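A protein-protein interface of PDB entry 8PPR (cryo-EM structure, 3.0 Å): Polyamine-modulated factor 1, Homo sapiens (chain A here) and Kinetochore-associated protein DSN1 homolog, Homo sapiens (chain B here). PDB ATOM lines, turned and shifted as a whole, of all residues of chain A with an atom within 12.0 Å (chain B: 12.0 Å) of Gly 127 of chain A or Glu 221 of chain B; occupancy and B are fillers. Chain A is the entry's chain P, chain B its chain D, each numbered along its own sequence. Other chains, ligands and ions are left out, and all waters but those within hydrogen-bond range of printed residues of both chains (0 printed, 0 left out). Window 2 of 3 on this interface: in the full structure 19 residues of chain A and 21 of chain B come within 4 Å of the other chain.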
ATOM      1  N   ALA A 122      31.782 -11.786   4.806  1.00  0.00           N
ATOM      2  CA  ALA A 122      31.148 -10.937   3.815  1.00  0.00           C
ATOM      3  C   ALA A 122      29.930 -11.635   3.217  1.00  0.00           C
ATOM      4  O   ALA A 122      29.734 -12.845   3.360  1.00  0.00           O
ATOM      5  CB  ALA A 122      32.140 -10.554   2.718  1.00  0.00           C
ATOM      6  N   TRP A 123      29.100 -10.848   2.538  1.00  0.00           N
ATOM      7  CA  TRP A 123      27.898 -11.383   1.919  1.00  0.00           C
ATOM      8  C   TRP A 123      28.256 -12.344   0.794  1.00  0.00           C
ATOM      9  O   TRP A 123      29.252 -12.171   0.087  1.00  0.00           O
ATOM     10  CB  TRP A 123      27.025 -10.249   1.383  1.00  0.00           C
ATOM     11  CG  TRP A 123      25.768 -10.718   0.718  1.00  0.00           C
ATOM     12  CD1 TRP A 123      24.551 -10.903   1.305  1.00  0.00           C
ATOM     13  CD2 TRP A 123      25.603 -11.059  -0.662  1.00  0.00           C
ATOM     14  NE1 TRP A 123      23.638 -11.338   0.376  1.00  0.00           N
ATOM     15  CE2 TRP A 123      24.259 -11.443  -0.841  1.00  0.00           C
ATOM     16  CE3 TRP A 123      26.462 -11.079  -1.765  1.00  0.00           C
ATOM     17  CZ2 TRP A 123      23.754 -11.841  -2.076  1.00  0.00           C
ATOM     18  CZ3 TRP A 123      25.959 -11.475  -2.990  1.00  0.00           C
ATOM     19  CH2 TRP A 123      24.618 -11.848  -3.136  1.00  0.00           C
ATOM     20  N   ARG A 124      27.433 -13.369   0.637  1.00  0.00           N
ATOM     21  CA  ARG A 124      27.605 -14.389  -0.383  1.00  0.00           C
ATOM     22  C   ARG A 124      26.282 -14.598  -1.097  1.00  0.00           C
ATOM     23  O   ARG A 124      25.218 -14.300  -0.543  1.00  0.00           O
ATOM     24  CB  ARG A 124      28.091 -15.709   0.235  1.00  0.00           C
ATOM     25  CG  ARG A 124      29.492 -15.617   0.807  1.00  0.00           C
ATOM     26  CD  ARG A 124      30.479 -15.157  -0.253  1.00  0.00           C
ATOM     27  NE  ARG A 124      31.860 -15.416   0.132  1.00  0.00           N
ATOM     28  CZ  ARG A 124      32.700 -14.487   0.567  1.00  0.00           C
ATOM     29  NH1 ARG A 124      32.329 -13.224   0.692  1.00  0.00           N
ATOM     30  NH2 ARG A 124      33.944 -14.835   0.884  1.00  0.00           N
ATOM     31  N   PRO A 125      26.312 -15.084  -2.339  1.00  0.00           N
ATOM     32  CA  PRO A 125      25.059 -15.285  -3.076  1.00  0.00           C
ATOM     33  C   PRO A 125      24.103 -16.195  -2.320  1.00  0.00           C
ATOM     34  O   PRO A 125      24.493 -17.234  -1.783  1.00  0.00           O
ATOM     35  CB  PRO A 125      25.522 -15.919  -4.393  1.00  0.00           C
ATOM     36  CG  PRO A 125      26.923 -15.439  -4.559  1.00  0.00           C
ATOM     37  CD  PRO A 125      27.493 -15.374  -3.172  1.00  0.00           C
ATOM     38  N   SER A 126      22.836 -15.786  -2.284  1.00  0.00           N
ATOM     39  CA  SER A 126      21.822 -16.536  -1.554  1.00  0.00           C
ATOM     40  C   SER A 126      21.407 -17.803  -2.288  1.00  0.00           C
ATOM     41  O   SER A 126      20.954 -18.761  -1.653  1.00  0.00           O
ATOM     42  CB  SER A 126      20.601 -15.653  -1.306  1.00  0.00           C
ATOM     43  OG  SER A 126      19.762 -15.623  -2.447  1.00  0.00           O
ATOM     44  N   GLY A 127      21.550 -17.826  -3.609  1.00  0.00           N
ATOM     45  CA  GLY A 127      21.068 -18.917  -4.427  1.00  0.00           C
ATOM     46  C   GLY A 127      19.751 -18.630  -5.107  1.00  0.00           C
ATOM     47  O   GLY A 127      19.410 -19.314  -6.079  1.00  0.00           O
ATOM     48  N   ILE A 128      19.004 -17.640  -4.631  1.00  0.00           N
ATOM     49  CA  ILE A 128      17.770 -17.194  -5.261  1.00  0.00           C
ATOM     50  C   ILE A 128      18.018 -15.808  -5.846  1.00  0.00           C
ATOM     51  O   ILE A 128      18.463 -14.902  -5.134  1.00  0.00           O
ATOM     52  CB  ILE A 128      16.574 -17.195  -4.289  1.00  0.00           C
ATOM     53  CG1 ILE A 128      15.261 -17.021  -5.057  1.00  0.00           C
ATOM     54  CG2 ILE A 128      16.729 -16.173  -3.166  1.00  0.00           C
ATOM     55  CD1 ILE A 128      14.931 -18.182  -5.969  1.00  0.00           C
ATOM     56  N   PRO A 129      17.828 -15.614  -7.152  1.00  0.00           N
ATOM     57  CA  PRO A 129      18.148 -14.311  -7.757  1.00  0.00           C
ATOM     58  C   PRO A 129      17.329 -13.150  -7.216  1.00  0.00           C
ATOM     59  O   PRO A 129      17.806 -12.011  -7.264  1.00  0.00           O
ATOM     60  CB  PRO A 129      17.866 -14.545  -9.247  1.00  0.00           C
ATOM     61  CG  PRO A 129      18.045 -16.014  -9.434  1.00  0.00           C
ATOM     62  CD  PRO A 129      17.525 -16.636  -8.167  1.00  0.00           C
ATOM     63  N   GLU A 130      16.116 -13.391  -6.714  1.00  0.00           N
ATOM     64  CA  GLU A 130      15.252 -12.283  -6.310  1.00  0.00           C
ATOM     65  C   GLU A 130      15.828 -11.531  -5.117  1.00  0.00           C
ATOM     66  O   GLU A 130      15.946 -10.299  -5.142  1.00  0.00           O
ATOM     67  CB  GLU A 130      13.851 -12.802  -5.992  1.00  0.00           C
ATOM     68  CG  GLU A 130      13.104 -13.337  -7.197  1.00  0.00           C
ATOM     69  CD  GLU A 130      11.726 -13.851  -6.841  1.00  0.00           C
ATOM     70  OE1 GLU A 130      11.406 -13.907  -5.636  1.00  0.00           O
ATOM     71  OE2 GLU A 130      10.960 -14.194  -7.766  1.00  0.00           O
ATOM     72  N   LYS A 131      16.192 -12.254  -4.058  1.00  0.00           N
ATOM     73  CA  LYS A 131      16.769 -11.597  -2.892  1.00  0.00           C
ATOM     74  C   LYS A 131      18.145 -11.026  -3.197  1.00  0.00           C
ATOM     75  O   LYS A 131      18.547 -10.026  -2.593  1.00  0.00           O
ATOM     76  CB  LYS A 131      16.834 -12.573  -1.719  1.00  0.00           C
ATOM     77  CG  LYS A 131      15.678 -12.425  -0.743  1.00  0.00           C
ATOM     78  CD  LYS A 131      14.338 -12.677  -1.416  1.00  0.00           C
ATOM     79  CE  LYS A 131      14.152 -14.141  -1.767  1.00  0.00           C
ATOM     80  NZ  LYS A 131      12.782 -14.418  -2.278  1.00  0.00           N
ATOM     81  N   ASP A 132      18.875 -11.642  -4.126  1.00  0.00           N
ATOM     82  CA  ASP A 132      20.162 -11.094  -4.534  1.00  0.00           C
ATOM     83  C   ASP A 132      19.988  -9.754  -5.241  1.00  0.00           C
ATOM     84  O   ASP A 132      20.757  -8.816  -5.005  1.00  0.00           O
ATOM     85  CB  ASP A 132      20.887 -12.090  -5.437  1.00  0.00           C
ATOM     86  CG  ASP A 132      21.174 -13.405  -4.741  1.00  0.00           C
ATOM     87  OD1 ASP A 132      21.320 -13.402  -3.501  1.00  0.00           O
ATOM     88  OD2 ASP A 132      21.247 -14.443  -5.432  1.00  0.00           O
ATOM     89  N   LEU A 133      18.977  -9.645  -6.099  1.00  0.00           N
ATOM     90  CA  LEU A 133      18.715  -8.434  -6.864  1.00  0.00           C
ATOM     91  C   LEU A 133      17.972  -7.374  -6.064  1.00  0.00           C
ATOM     92  O   LEU A 133      17.943  -6.209  -6.483  1.00  0.00           O
ATOM     93  CB  LEU A 133      17.908  -8.779  -8.121  1.00  0.00           C
ATOM     94  CG  LEU A 133      18.679  -9.405  -9.286  1.00  0.00           C
ATOM     95  CD1 LEU A 133      17.826  -9.429 -10.544  1.00  0.00           C
ATOM     96  CD2 LEU A 133      19.977  -8.656  -9.534  1.00  0.00           C
ATOM     97  N   HIS A 134      17.362  -7.758  -4.941  1.00  0.00           N
ATOM     98  CA  HIS A 134      16.643  -6.790  -4.120  1.00  0.00           C
ATOM     99  C   HIS A 134      17.572  -5.692  -3.619  1.00  0.00           C
ATOM    100  O   HIS A 134      17.225  -4.507  -3.663  1.00  0.00           O
ATOM    101  CB  HIS A 134      15.974  -7.503  -2.946  1.00  0.00           C
ATOM    102  CG  HIS A 134      14.676  -8.159  -3.298  1.00  0.00           C
ATOM    103  ND1 HIS A 134      13.983  -7.864  -4.452  1.00  0.00           N
ATOM    104  CD2 HIS A 134      13.953  -9.107  -2.657  1.00  0.00           C
ATOM    105  CE1 HIS A 134      12.884  -8.594  -4.501  1.00  0.00           C
ATOM    106  NE2 HIS A 134      12.842  -9.357  -3.424  1.00  0.00           N
ATOM    107  N   LYS B 212      25.419 -34.042  -8.241  1.00  0.00           N
ATOM    108  CA  LYS B 212      24.111 -34.025  -8.886  1.00  0.00           C
ATOM    109  C   LYS B 212      23.189 -33.012  -8.225  1.00  0.00           C
ATOM    110  O   LYS B 212      22.504 -32.242  -8.911  1.00  0.00           O
ATOM    111  CB  LYS B 212      23.492 -35.421  -8.845  1.00  0.00           C
ATOM    112  CG  LYS B 212      22.182 -35.540  -9.601  1.00  0.00           C
ATOM    113  CD  LYS B 212      21.285 -36.592  -8.971  1.00  0.00           C
ATOM    114  CE  LYS B 212      19.848 -36.449  -9.442  1.00  0.00           C
ATOM    115  NZ  LYS B 212      19.386 -35.035  -9.383  1.00  0.00           N
ATOM    116  N   GLU B 213      23.172 -32.987  -6.891  1.00  0.00           N
ATOM    117  CA  GLU B 213      22.367 -31.996  -6.187  1.00  0.00           C
ATOM    118  C   GLU B 213      22.809 -30.582  -6.540  1.00  0.00           C
ATOM    119  O   GLU B 213      21.974 -29.706  -6.804  1.00  0.00           O
ATOM    120  CB  GLU B 213      22.459 -32.224  -4.681  1.00  0.00           C
ATOM    121  CG  GLU B 213      21.739 -31.178  -3.857  1.00  0.00           C
ATOM    122  CD  GLU B 213      21.614 -31.576  -2.404  1.00  0.00           C
ATOM    123  OE1 GLU B 213      21.924 -32.741  -2.078  1.00  0.00           O
ATOM    124  OE2 GLU B 213      21.209 -30.724  -1.587  1.00  0.00           O
ATOM    125  N   TYR B 214      24.122 -30.345  -6.561  1.00  0.00           N
ATOM    126  CA  TYR B 214      24.633 -29.013  -6.858  1.00  0.00           C
ATOM    127  C   TYR B 214      24.270 -28.579  -8.271  1.00  0.00           C
ATOM    128  O   TYR B 214      23.843 -27.439  -8.485  1.00  0.00           O
ATOM    129  CB  TYR B 214      26.147 -28.977  -6.662  1.00  0.00           C
ATOM    130  CG  TYR B 214      26.586 -29.122  -5.224  1.00  0.00           C
ATOM    131  CD1 TYR B 214      25.683 -28.969  -4.182  1.00  0.00           C
ATOM    132  CD2 TYR B 214      27.906 -29.412  -4.909  1.00  0.00           C
ATOM    133  CE1 TYR B 214      26.082 -29.102  -2.866  1.00  0.00           C
ATOM    134  CE2 TYR B 214      28.315 -29.547  -3.597  1.00  0.00           C
ATOM    135  CZ  TYR B 214      27.400 -29.391  -2.580  1.00  0.00           C
ATOM    136  OH  TYR B 214      27.803 -29.524  -1.272  1.00  0.00           O
ATOM    137  N   ILE B 215      24.435 -29.470  -9.252  1.00  0.00           N
ATOM    138  CA  ILE B 215      24.153 -29.093 -10.632  1.00  0.00           C
ATOM    139  C   ILE B 215      22.660 -28.876 -10.834  1.00  0.00           C
ATOM    140  O   ILE B 215      22.254 -27.987 -11.588  1.00  0.00           O
ATOM    141  CB  ILE B 215      24.725 -30.125 -11.625  1.00  0.00           C
ATOM    142  CG1 ILE B 215      24.077 -31.497 -11.449  1.00  0.00           C
ATOM    143  CG2 ILE B 215      26.239 -30.210 -11.502  1.00  0.00           C
ATOM    144  CD1 ILE B 215      24.472 -32.498 -12.512  1.00  0.00           C
ATOM    145  N   THR B 216      21.814 -29.667 -10.165  1.00  0.00           N
ATOM    146  CA  THR B 216      20.378 -29.419 -10.249  1.00  0.00           C
ATOM    147  C   THR B 216      20.021 -28.060  -9.657  1.00  0.00           C
ATOM    148  O   THR B 216      19.259 -27.287 -10.258  1.00  0.00           O
ATOM    149  CB  THR B 216      19.606 -30.527  -9.534  1.00  0.00           C
ATOM    150  OG1 THR B 216      20.222 -30.801  -8.270  1.00  0.00           O
ATOM    151  CG2 THR B 216      19.596 -31.794 -10.374  1.00  0.00           C
ATOM    152  N   LYS B 217      20.579 -27.746  -8.485  1.00  0.00           N
ATOM    153  CA  LYS B 217      20.313 -26.456  -7.859  1.00  0.00           C
ATOM    154  C   LYS B 217      20.762 -25.313  -8.756  1.00  0.00           C
ATOM    155  O   LYS B 217      20.046 -24.319  -8.924  1.00  0.00           O
ATOM    156  CB  LYS B 217      21.021 -26.384  -6.510  1.00  0.00           C
ATOM    157  CG  LYS B 217      20.293 -27.087  -5.381  1.00  0.00           C
ATOM    158  CD  LYS B 217      20.931 -26.756  -4.045  1.00  0.00           C
ATOM    159  CE  LYS B 217      22.424 -27.047  -4.071  1.00  0.00           C
ATOM    160  NZ  LYS B 217      23.076 -26.764  -2.764  1.00  0.00           N
ATOM    161  N   PHE B 218      21.940 -25.450  -9.363  1.00  0.00           N
ATOM    162  CA  PHE B 218      22.475 -24.381 -10.195  1.00  0.00           C
ATOM    163  C   PHE B 218      21.718 -24.263 -11.510  1.00  0.00           C
ATOM    164  O   PHE B 218      21.590 -23.160 -12.050  1.00  0.00           O
ATOM    165  CB  PHE B 218      23.963 -24.624 -10.435  1.00  0.00           C
ATOM    166  CG  PHE B 218      24.781 -24.581  -9.179  1.00  0.00           C
ATOM    167  CD1 PHE B 218      24.346 -23.853  -8.083  1.00  0.00           C
ATOM    168  CD2 PHE B 218      25.963 -25.293  -9.077  1.00  0.00           C
ATOM    169  CE1 PHE B 218      25.086 -23.818  -6.918  1.00  0.00           C
ATOM    170  CE2 PHE B 218      26.704 -25.264  -7.911  1.00  0.00           C
ATOM    171  CZ  PHE B 218      26.266 -24.524  -6.832  1.00  0.00           C
ATOM    172  N   SER B 219      21.206 -25.379 -12.035  1.00  0.00           N
ATOM    173  CA  SER B 219      20.359 -25.319 -13.221  1.00  0.00           C
ATOM    174  C   SER B 219      19.065 -24.573 -12.928  1.00  0.00           C
ATOM    175  O   SER B 219      18.634 -23.726 -13.719  1.00  0.00           O
ATOM    176  CB  SER B 219      20.067 -26.731 -13.727  1.00  0.00           C
ATOM    177  OG  SER B 219      21.251 -27.364 -14.180  1.00  0.00           O
ATOM    178  N   LEU B 220      18.436 -24.864 -11.786  1.00  0.00           N
ATOM    179  CA  LEU B 220      17.264 -24.086 -11.395  1.00  0.00           C
ATOM    180  C   LEU B 220      17.620 -22.617 -11.200  1.00  0.00           C
ATOM    181  O   LEU B 220      16.840 -21.728 -11.565  1.00  0.00           O
ATOM    182  CB  LEU B 220      16.625 -24.665 -10.132  1.00  0.00           C
ATOM    183  CG  LEU B 220      15.651 -25.842 -10.277  1.00  0.00           C
ATOM    184  CD1 LEU B 220      14.431 -25.394 -11.067  1.00  0.00           C
ATOM    185  CD2 LEU B 220      16.273 -27.065 -10.928  1.00  0.00           C
ATOM    186  N   GLU B 221      18.797 -22.342 -10.635  1.00  0.00           N
ATOM    187  CA  GLU B 221      19.204 -20.956 -10.419  1.00  0.00           C
ATOM    188  C   GLU B 221      19.377 -20.207 -11.736  1.00  0.00           C
ATOM    189  O   GLU B 221      18.911 -19.071 -11.872  1.00  0.00           O
ATOM    190  CB  GLU B 221      20.495 -20.908  -9.607  1.00  0.00           C
ATOM    191  CG  GLU B 221      21.008 -19.500  -9.363  1.00  0.00           C
ATOM    192  CD  GLU B 221      21.913 -19.416  -8.153  1.00  0.00           C
ATOM    193  OE1 GLU B 221      21.814 -20.296  -7.274  1.00  0.00           O
ATOM    194  OE2 GLU B 221      22.725 -18.469  -8.082  1.00  0.00           O
ATOM    195  N   ARG B 222      20.044 -20.821 -12.717  1.00  0.00           N
ATOM    196  CA  ARG B 222      20.229 -20.146 -13.998  1.00  0.00           C
ATOM    197  C   ARG B 222      18.911 -20.014 -14.748  1.00  0.00           C
ATOM    198  O   ARG B 222      18.696 -19.017 -15.447  1.00  0.00           O
ATOM    199  CB  ARG B 222      21.253 -20.877 -14.866  1.00  0.00           C
ATOM    200  CG  ARG B 222      21.037 -22.363 -14.989  1.00  0.00           C
ATOM    201  CD  ARG B 222      21.841 -22.955 -16.126  1.00  0.00           C
ATOM    202  NE  ARG B 222      21.455 -22.394 -17.414  1.00  0.00           N
ATOM    203  CZ  ARG B 222      22.090 -22.634 -18.553  1.00  0.00           C
ATOM    204  NH1 ARG B 222      23.149 -23.426 -18.601  1.00  0.00           N
ATOM    205  NH2 ARG B 222      21.649 -22.067 -19.672  1.00  0.00           N
ATOM    206  N   GLN B 223      18.022 -21.001 -14.620  1.00  0.00           N
ATOM    207  CA  GLN B 223      16.695 -20.871 -15.210  1.00  0.00           C
ATOM    208  C   GLN B 223      15.948 -19.687 -14.612  1.00  0.00           C
ATOM    209  O   GLN B 223      15.333 -18.899 -15.338  1.00  0.00           O
ATOM    210  CB  GLN B 223      15.909 -22.164 -15.005  1.00  0.00           C
ATOM    211  CG  GLN B 223      16.352 -23.302 -15.903  1.00  0.00           C
ATOM    212  CD  GLN B 223      15.647 -24.602 -15.576  1.00  0.00           C
ATOM    213  OE1 GLN B 223      14.961 -24.709 -14.560  1.00  0.00           O
ATOM    214  NE2 GLN B 223      15.815 -25.599 -16.435  1.00  0.00           N
ATOM    215  N   THR B 224      16.000 -19.542 -13.286  1.00  0.00           N
ATOM    216  CA  THR B 224      15.353 -18.409 -12.634  1.00  0.00           C
ATOM    217  C   THR B 224      15.991 -17.093 -13.061  1.00  0.00           C
ATOM    218  O   THR B 224      15.295 -16.089 -13.254  1.00  0.00           O
ATOM    219  CB  THR B 224      15.423 -18.572 -11.117  1.00  0.00           C
ATOM    220  OG1 THR B 224      14.799 -19.806 -10.741  1.00  0.00           O
ATOM    221  CG2 THR B 224      14.710 -17.423 -10.422  1.00  0.00           C
ATOM    222  N   TRP B 225      17.317 -17.079 -13.205  1.00  0.00           N
ATOM    223  CA  TRP B 225      18.012 -15.884 -13.670  1.00  0.00           C
ATOM    224  C   TRP B 225      17.538 -15.481 -15.060  1.00  0.00           C
ATOM    225  O   TRP B 225      17.259 -14.303 -15.323  1.00  0.00           O
ATOM    226  CB  TRP B 225      19.517 -16.138 -13.675  1.00  0.00           C
ATOM    227  CG  TRP B 225      20.203 -15.764 -12.411  1.00  0.00           C
ATOM    228  CD1 TRP B 225      20.841 -16.602 -11.545  1.00  0.00           C
ATOM    229  CD2 TRP B 225      20.342 -14.446 -11.872  1.00  0.00           C
ATOM    230  NE1 TRP B 225      21.361 -15.888 -10.493  1.00  0.00           N
ATOM    231  CE2 TRP B 225      21.068 -14.560 -10.671  1.00  0.00           C
ATOM    232  CE3 TRP B 225      19.916 -13.181 -12.286  1.00  0.00           C
ATOM    233  CZ2 TRP B 225      21.379 -13.458  -9.881  1.00  0.00           C
ATOM    234  CZ3 TRP B 225      20.227 -12.088 -11.502  1.00  0.00           C
ATOM    235  CH2 TRP B 225      20.951 -12.233 -10.313  1.00  0.00           C
ATOM    236  N   ASP B 226      17.445 -16.454 -15.965  1.00  0.00           N
ATOM    237  CA  ASP B 226      16.983 -16.171 -17.318  1.00  0.00           C
ATOM    238  C   ASP B 226      15.538 -15.695 -17.313  1.00  0.00           C
ATOM    239  O   ASP B 226      15.177 -14.779 -18.062  1.00  0.00           O
ATOM    240  CB  ASP B 226      17.142 -17.415 -18.189  1.00  0.00           C
ATOM    241  CG  ASP B 226      18.596 -17.762 -18.445  1.00  0.00           C
ATOM    242  OD1 ASP B 226      19.425 -16.831 -18.525  1.00  0.00           O
ATOM    243  OD2 ASP B 226      18.910 -18.965 -18.559  1.00  0.00           O
ATOM    244  N   GLN B 227      14.696 -16.307 -16.475  1.00  0.00           N
ATOM    245  CA  GLN B 227      13.308 -15.872 -16.371  1.00  0.00           C
ATOM    246  C   GLN B 227      13.216 -14.434 -15.881  1.00  0.00           C
ATOM    247  O   GLN B 227      12.432 -13.640 -16.410  1.00  0.00           O
ATOM    248  CB  GLN B 227      12.528 -16.803 -15.443  1.00  0.00           C
ATOM    249  CG  GLN B 227      12.358 -18.211 -15.978  1.00  0.00           C
ATOM    250  CD  GLN B 227      11.739 -18.236 -17.360  1.00  0.00           C
ATOM    251  OE1 GLN B 227      10.825 -17.468 -17.659  1.00  0.00           O
ATOM    252  NE2 GLN B 227      12.239 -19.121 -18.214  1.00  0.00           N
ATOM    253  N   LEU B 228      14.010 -14.083 -14.870  1.00  0.00           N
ATOM    254  CA  LEU B 228      13.999 -12.716 -14.363  1.00  0.00           C
ATOM    255  C   LEU B 228      14.464 -11.733 -15.427  1.00  0.00           C
ATOM    256  O   LEU B 228      13.864 -10.665 -15.606  1.00  0.00           O
ATOM    257  CB  LEU B 228      14.879 -12.616 -13.118  1.00  0.00           C
ATOM    258  CG  LEU B 228      14.267 -13.171 -11.832  1.00  0.00           C
ATOM    259  CD1 LEU B 228      15.062 -12.721 -10.619  1.00  0.00           C
ATOM    260  CD2 LEU B 228      12.809 -12.760 -11.709  1.00  0.00           C
ATOM    261  N   LEU B 229      15.534 -12.081 -16.147  1.00  0.00           N
ATOM    262  CA  LEU B 229      16.035 -11.199 -17.195  1.00  0.00           C
ATOM    263  C   LEU B 229      14.993 -10.986 -18.284  1.00  0.00           C
ATOM    264  O   LEU B 229      14.746  -9.848 -18.703  1.00  0.00           O
ATOM    265  CB  LEU B 229      17.321 -11.768 -17.790  1.00  0.00           C
ATOM    266  CG  LEU B 229      18.074 -10.850 -18.756  1.00  0.00           C
ATOM    267  CD1 LEU B 229      19.566 -10.913 -18.497  1.00  0.00           C
ATOM    268  CD2 LEU B 229      17.770 -11.219 -20.203  1.00  0.00           C
ATOM    269  N   LEU B 230      14.372 -12.071 -18.757  1.00  0.00           N
ATOM    270  CA  LEU B 230      13.376 -11.935 -19.813  1.00  0.00           C
ATOM    271  C   LEU B 230      12.162 -11.160 -19.320  1.00  0.00           C
ATOM    272  O   LEU B 230      11.614 -10.329 -20.050  1.00  0.00           O
ATOM    273  CB  LEU B 230      12.974 -13.309 -20.356  1.00  0.00           C
ATOM    274  CG  LEU B 230      12.291 -14.369 -19.487  1.00  0.00           C
ATOM    275  CD1 LEU B 230      10.776 -14.197 -19.452  1.00  0.00           C
ATOM    276  CD2 LEU B 230      12.659 -15.762 -19.973  1.00  0.00           C
ATOM    277  N   TYR B 232      12.080  -8.789 -16.989  1.00  0.00           N
ATOM    278  CA  TYR B 232      12.379  -7.368 -16.856  1.00  0.00           C
ATOM    279  C   TYR B 232      12.559  -6.705 -18.214  1.00  0.00           C
ATOM    280  O   TYR B 232      12.065  -5.591 -18.433  1.00  0.00           O
ATOM    281  CB  TYR B 232      13.607  -7.186 -15.971  1.00  0.00           C
ATOM    282  CG  TYR B 232      13.323  -7.574 -14.541  1.00  0.00           C
ATOM    283  CD1 TYR B 232      12.016  -7.736 -14.096  1.00  0.00           C
ATOM    284  CD2 TYR B 232      14.351  -7.796 -13.642  1.00  0.00           C
ATOM    285  CE1 TYR B 232      11.744  -8.096 -12.796  1.00  0.00           C
ATOM    286  CE2 TYR B 232      14.088  -8.157 -12.336  1.00  0.00           C
ATOM    287  CZ  TYR B 232      12.782  -8.306 -11.917  1.00  0.00           C
ATOM    288  OH  TYR B 232      12.516  -8.666 -10.617  1.00  0.00           O
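O of Gly 127 of chain A lies close to OE1 of Glu 221 of chain B (2.9 Å).
O of Glu 130 of chain A lies close to ND1 of His 134 of chain A (3.2 Å).
The side-chain carboxylate of Glu 130 of chain A lies within salt-bridge range of the side-chain amino group of Lys 131 of chain A (3.7 Å).
The backbone carbonyl oxygen (O) of Leu 220 of chain B sits at hydrogen-bond distance from the side-chain hydroxyl (OG1) of Thr 224 of chain B (2.9 Å).
Among the printed residues, merely in contact across the chains: Pro 129 of chain A with Trp 225 of chain B (3.5 Å), Pro 129 of chain A with Leu 228 of chain B (3.6 Å), Pro 129 of chain A with Thr 224 of chain B (3.7 Å), Leu 133 of chain A with Trp 225 of chain B (3.7 Å) and Glu 130 of chain A with Leu 228 of chain B (3.99 Å).
No residue of chain B comes within 4 Å of Ser 126 of chain A.
No residue of chain B comes within 4 Å of Ile 128 of chain A.
Of the printed residues of chain B, Pro 129 of chain A touches Thr 224 (3.7 Å), Trp 225 (3.5 Å) and Leu 228 (3.6 Å).
No residue of chain A comes within 4 Å of Phe 218 of chain B.
Of the printed residues of chain A, Glu 221 of chain B touches Gly 127 (2.9 Å).
No residue of chain A comes within 4 Å of Gln 223 of chain B.
Thr 224 of chain B touches just one residue of chain A: Pro 129.
Trp 225 of chain B touches just these residues of chain A: Pro 129 and Leu 133.
Asp 226 of chain B touches none of the printed residues of chain A.
Of the printed residues of chain A, Leu 228 of chain B touches Pro 129 (3.6 Å) and Glu 130 (3.99 Å).
The nearest printed residue of chain A that does not touch Glu 221 of chain B is Pro 129 of chain A (4.005 Å).
Of the 20 printed residues of chain B, 4 touch a printed residue of chain A.
Printed residues of chain B that touch a printed residue of chain A: Glu 221, Thr 224, Trp 225 and Leu 228.
Of the 13 printed residues of chain A, 4 touch a printed residue of chain B.
Along chain A the printed residues that touch a printed residue of chain B span positions 127 to 133.
Among the printed residues, 6 pairs touch across the chains.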
